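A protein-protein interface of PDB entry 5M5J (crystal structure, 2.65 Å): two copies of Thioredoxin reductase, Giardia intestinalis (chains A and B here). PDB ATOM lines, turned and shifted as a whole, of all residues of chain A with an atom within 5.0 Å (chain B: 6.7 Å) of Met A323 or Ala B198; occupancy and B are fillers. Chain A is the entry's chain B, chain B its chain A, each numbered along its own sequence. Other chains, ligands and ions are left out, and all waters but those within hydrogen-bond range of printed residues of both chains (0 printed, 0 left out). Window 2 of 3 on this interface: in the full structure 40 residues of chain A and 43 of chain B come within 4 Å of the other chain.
Of the 10 printed residues of chain B, 4 touch a printed residue of chain A.
Hydrophobic or aromatic side chains of chain A that line the printed part of chain B: Ala A322 and Met A323.
Among the printed residues, Asp or Glu carboxylates within 4 Å of a Lys or Arg side-chain nitrogen of the other chain: Glu A325 with Lys B202.
The side-chain carboxylate (OE1) of Glu A325 lies within salt-bridge range of the side-chain amino group (NZ) of Lys B202 (3.8 Å).
NZ of Lys B202 lies within hydrogen-bond range of O of Ala A322 (2.6 Å).
No position is printed for both chains.
Of the 6 pairs that touch across the chains among the printed residues, none has its exchanged pair printed and touching as well.
Of the printed residues of chain B, Glu A325 touches Lys B202 (3.4 Å).
Ala B197 touches none of the printed residues of chain A.
Of the printed residues of chain A, Ala B198 touches Met A323 (3.9 Å).
Printed residues of chain A within 4 Å of Lys B202: Ala A322 (2.6 Å), Met A323 (3.97 Å) and Glu A325 (3.4 Å).
CB of Ala A322 touches CG2 of Thr B175, 3.9 Å away.
Met A323 touches Ala B198.
SD of Met B199 touches SD of Met A323, 3.9 Å away.
Lys B202 touches Met A323.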
ATOM      1  N   ARG A 319      19.009   3.371   5.498  1.00  0.00           N
ATOM      2  CA  ARG A 319      17.972   3.103   6.493  1.00  0.00           C
ATOM      3  C   ARG A 319      18.542   2.540   7.767  1.00  0.00           C
ATOM      4  O   ARG A 319      18.132   2.935   8.839  1.00  0.00           O
ATOM      5  CB  ARG A 319      16.929   2.128   5.959  1.00  0.00           C
ATOM      6  CG  ARG A 319      15.902   2.794   5.071  1.00  0.00           C
ATOM      7  CD  ARG A 319      15.287   1.790   4.119  1.00  0.00           C
ATOM      8  NE  ARG A 319      14.737   2.443   2.936  1.00  0.00           N
ATOM      9  CZ  ARG A 319      14.360   1.812   1.829  1.00  0.00           C
ATOM     10  NH1 ARG A 319      14.465   0.487   1.716  1.00  0.00           N
ATOM     11  NH2 ARG A 319      13.875   2.523   0.821  1.00  0.00           N
ATOM     12  N   TRP A 320      19.476   1.607   7.639  1.00  0.00           N
ATOM     13  CA  TRP A 320      20.098   0.993   8.798  1.00  0.00           C
ATOM     14  C   TRP A 320      20.886   2.027   9.592  1.00  0.00           C
ATOM     15  O   TRP A 320      20.715   2.113  10.809  1.00  0.00           O
ATOM     16  CB  TRP A 320      20.992  -0.176   8.388  1.00  0.00           C
ATOM     17  CG  TRP A 320      21.630  -0.859   9.562  1.00  0.00           C
ATOM     18  CD1 TRP A 320      21.058  -1.788  10.389  1.00  0.00           C
ATOM     19  CD2 TRP A 320      22.958  -0.651  10.048  1.00  0.00           C
ATOM     20  NE1 TRP A 320      21.956  -2.174  11.358  1.00  0.00           N
ATOM     21  CE2 TRP A 320      23.129  -1.492  11.173  1.00  0.00           C
ATOM     22  CE3 TRP A 320      24.021   0.164   9.642  1.00  0.00           C
ATOM     23  CZ2 TRP A 320      24.324  -1.546  11.896  1.00  0.00           C
ATOM     24  CZ3 TRP A 320      25.216   0.112  10.357  1.00  0.00           C
ATOM     25  CH2 TRP A 320      25.353  -0.736  11.478  1.00  0.00           C
ATOM     26  N   LEU A 321      21.715   2.824   8.911  1.00  0.00           N
ATOM     27  CA  LEU A 321      22.486   3.882   9.580  1.00  0.00           C
ATOM     28  C   LEU A 321      21.589   4.862  10.316  1.00  0.00           C
ATOM     29  O   LEU A 321      21.864   5.208  11.455  1.00  0.00           O
ATOM     30  CB  LEU A 321      23.369   4.653   8.596  1.00  0.00           C
ATOM     31  CG  LEU A 321      24.646   3.944   8.146  1.00  0.00           C
ATOM     32  CD1 LEU A 321      25.230   4.626   6.916  1.00  0.00           C
ATOM     33  CD2 LEU A 321      25.668   3.898   9.274  1.00  0.00           C
ATOM     34  N   ALA A 322      20.514   5.289   9.655  1.00  0.00           N
ATOM     35  CA  ALA A 322      19.579   6.268  10.214  1.00  0.00           C
ATOM     36  C   ALA A 322      18.885   5.763  11.483  1.00  0.00           C
ATOM     37  O   ALA A 322      18.704   6.523  12.430  1.00  0.00           O
ATOM     38  CB  ALA A 322      18.546   6.671   9.172  1.00  0.00           C
ATOM     39  N   MET A 323      18.507   4.490  11.516  1.00  0.00           N
ATOM     40  CA  MET A 323      17.903   3.931  12.722  1.00  0.00           C
ATOM     41  C   MET A 323      18.902   3.830  13.894  1.00  0.00           C
ATOM     42  O   MET A 323      18.474   3.824  15.038  1.00  0.00           O
ATOM     43  CB  MET A 323      17.236   2.577  12.439  1.00  0.00           C
ATOM     44  CG  MET A 323      16.088   2.597  11.417  1.00  0.00           C
ATOM     45  SD  MET A 323      14.763   3.827  11.615  1.00  0.00           S
ATOM     46  CE  MET A 323      14.278   3.540  13.321  1.00  0.00           C
ATOM     47  N   GLN A 324      20.210   3.775  13.612  1.00  0.00           N
ATOM     48  CA  GLN A 324      21.242   3.815  14.664  1.00  0.00           C
ATOM     49  C   GLN A 324      21.353   5.159  15.375  1.00  0.00           C
ATOM     50  O   GLN A 324      21.788   5.202  16.521  1.00  0.00           O
ATOM     51  CB  GLN A 324      22.636   3.452  14.124  1.00  0.00           C
ATOM     52  CG  GLN A 324      22.747   2.119  13.402  1.00  0.00           C
ATOM     53  CD  GLN A 324      21.922   1.031  14.061  1.00  0.00           C
ATOM     54  OE1 GLN A 324      22.194   0.653  15.199  1.00  0.00           O
ATOM     55  NE2 GLN A 324      20.901   0.538  13.363  1.00  0.00           N
ATOM     56  N   GLU A 325      20.977   6.247  14.711  1.00  0.00           N
ATOM     57  CA  GLU A 325      21.044   7.585  15.316  1.00  0.00           C
ATOM     58  C   GLU A 325      19.881   7.818  16.295  1.00  0.00           C
ATOM     59  O   GLU A 325      18.770   8.202  15.904  1.00  0.00           O
ATOM     60  CB  GLU A 325      21.050   8.665  14.233  1.00  0.00           C
ATOM     61  CG  GLU A 325      22.210   8.559  13.251  1.00  0.00           C
ATOM     62  CD  GLU A 325      22.120   9.585  12.133  1.00  0.00           C
ATOM     63  OE1 GLU A 325      21.047   9.685  11.494  1.00  0.00           O
ATOM     64  OE2 GLU A 325      23.125  10.289  11.881  1.00  0.00           O
ATOM     65  N   THR B 175      13.062  11.372   7.342  1.00  0.00           N
ATOM     66  CA  THR B 175      14.366  11.003   7.897  1.00  0.00           C
ATOM     67  C   THR B 175      15.494  11.135   6.872  1.00  0.00           C
ATOM     68  O   THR B 175      16.577  11.630   7.185  1.00  0.00           O
ATOM     69  CB  THR B 175      14.320   9.560   8.410  1.00  0.00           C
ATOM     70  OG1 THR B 175      13.204   9.425   9.289  1.00  0.00           O
ATOM     71  CG2 THR B 175      15.578   9.208   9.173  1.00  0.00           C
ATOM     72  N   ALA B 195       2.050   4.137  11.579  1.00  0.00           N
ATOM     73  CA  ALA B 195       3.387   3.667  11.265  1.00  0.00           C
ATOM     74  C   ALA B 195       3.929   2.826  12.420  1.00  0.00           C
ATOM     75  O   ALA B 195       3.368   2.827  13.522  1.00  0.00           O
ATOM     76  CB  ALA B 195       4.292   4.862  11.009  1.00  0.00           C
ATOM     77  N   SER B 196       5.035   2.129  12.158  1.00  0.00           N
ATOM     78  CA  SER B 196       5.708   1.302  13.155  1.00  0.00           C
ATOM     79  C   SER B 196       6.064   2.124  14.373  1.00  0.00           C
ATOM     80  O   SER B 196       6.374   3.304  14.255  1.00  0.00           O
ATOM     81  CB  SER B 196       6.999   0.713  12.591  1.00  0.00           C
ATOM     82  OG  SER B 196       6.907   0.517  11.195  1.00  0.00           O
ATOM     83  N   ALA B 197       6.035   1.487  15.539  1.00  0.00           N
ATOM     84  CA  ALA B 197       6.469   2.132  16.780  1.00  0.00           C
ATOM     85  C   ALA B 197       7.909   2.657  16.661  1.00  0.00           C
ATOM     86  O   ALA B 197       8.210   3.731  17.165  1.00  0.00           O
ATOM     87  CB  ALA B 197       6.337   1.172  17.958  1.00  0.00           C
ATOM     88  N   ALA B 198       8.772   1.909  15.967  1.00  0.00           N
ATOM     89  CA  ALA B 198      10.175   2.297  15.753  1.00  0.00           C
ATOM     90  C   ALA B 198      10.326   3.615  14.987  1.00  0.00           C
ATOM     91  O   ALA B 198      11.127   4.473  15.371  1.00  0.00           O
ATOM     92  CB  ALA B 198      10.917   1.187  15.019  1.00  0.00           C
ATOM     93  N   MET B 199       9.555   3.754  13.910  1.00  0.00           N
ATOM     94  CA  MET B 199       9.587   4.950  13.065  1.00  0.00           C
ATOM     95  C   MET B 199       9.037   6.180  13.765  1.00  0.00           C
ATOM     96  O   MET B 199       9.579   7.272  13.607  1.00  0.00           O
ATOM     97  CB  MET B 199       8.809   4.718  11.768  1.00  0.00           C
ATOM     98  CG  MET B 199       9.455   3.708  10.846  1.00  0.00           C
ATOM     99  SD  MET B 199      11.077   4.250  10.273  1.00  0.00           S
ATOM    100  CE  MET B 199      11.294   3.161   8.867  1.00  0.00           C
ATOM    101  N   VAL B 200       7.972   5.992  14.543  1.00  0.00           N
ATOM    102  CA  VAL B 200       7.324   7.092  15.268  1.00  0.00           C
ATOM    103  C   VAL B 200       8.261   7.641  16.343  1.00  0.00           C
ATOM    104  O   VAL B 200       8.356   8.860  16.510  1.00  0.00           O
ATOM    105  CB  VAL B 200       5.959   6.661  15.873  1.00  0.00           C
ATOM    106  CG1 VAL B 200       5.348   7.761  16.734  1.00  0.00           C
ATOM    107  CG2 VAL B 200       4.976   6.290  14.767  1.00  0.00           C
ATOM    108  N   LYS B 201       8.962   6.744  17.041  1.00  0.00           N
ATOM    109  CA  LYS B 201       9.955   7.127  18.059  1.00  0.00           C
ATOM    110  C   LYS B 201      11.097   7.937  17.444  1.00  0.00           C
ATOM    111  O   LYS B 201      11.428   9.015  17.932  1.00  0.00           O
ATOM    112  CB  LYS B 201      10.538   5.888  18.754  1.00  0.00           C
ATOM    113  CG  LYS B 201       9.549   5.099  19.612  1.00  0.00           C
ATOM    114  CD  LYS B 201       9.952   3.626  19.733  1.00  0.00           C
ATOM    115  CE  LYS B 201       8.815   2.743  20.241  1.00  0.00           C
ATOM    116  NZ  LYS B 201       8.461   3.022  21.660  1.00  0.00           N
ATOM    117  N   LYS B 202      11.681   7.395  16.375  1.00  0.00           N
ATOM    118  CA  LYS B 202      12.751   8.053  15.604  1.00  0.00           C
ATOM    119  C   LYS B 202      12.362   9.452  15.129  1.00  0.00           C
ATOM    120  O   LYS B 202      13.110  10.408  15.318  1.00  0.00           O
ATOM    121  CB  LYS B 202      13.125   7.189  14.392  1.00  0.00           C
ATOM    122  CG  LYS B 202      14.005   7.850  13.334  1.00  0.00           C
ATOM    123  CD  LYS B 202      15.413   8.147  13.823  1.00  0.00           C
ATOM    124  CE  LYS B 202      16.126   9.045  12.829  1.00  0.00           C
ATOM    125  NZ  LYS B 202      17.599   8.881  12.831  1.00  0.00           N
ATOM    126  N   VAL B 203      11.196   9.543  14.503  1.00  0.00           N
ATOM    127  CA  VAL B 203      10.684  10.803  13.962  1.00  0.00           C
ATOM    128  C   VAL B 203      10.419  11.856  15.059  1.00  0.00           C
ATOM    129  O   VAL B 203      10.736  13.037  14.880  1.00  0.00           O
ATOM    130  CB  VAL B 203       9.446  10.529  13.053  1.00  0.00           C
ATOM    131  CG1 VAL B 203       8.428  11.656  13.072  1.00  0.00           C
ATOM    132  CG2 VAL B 203       9.894  10.236  11.624  1.00  0.00           C
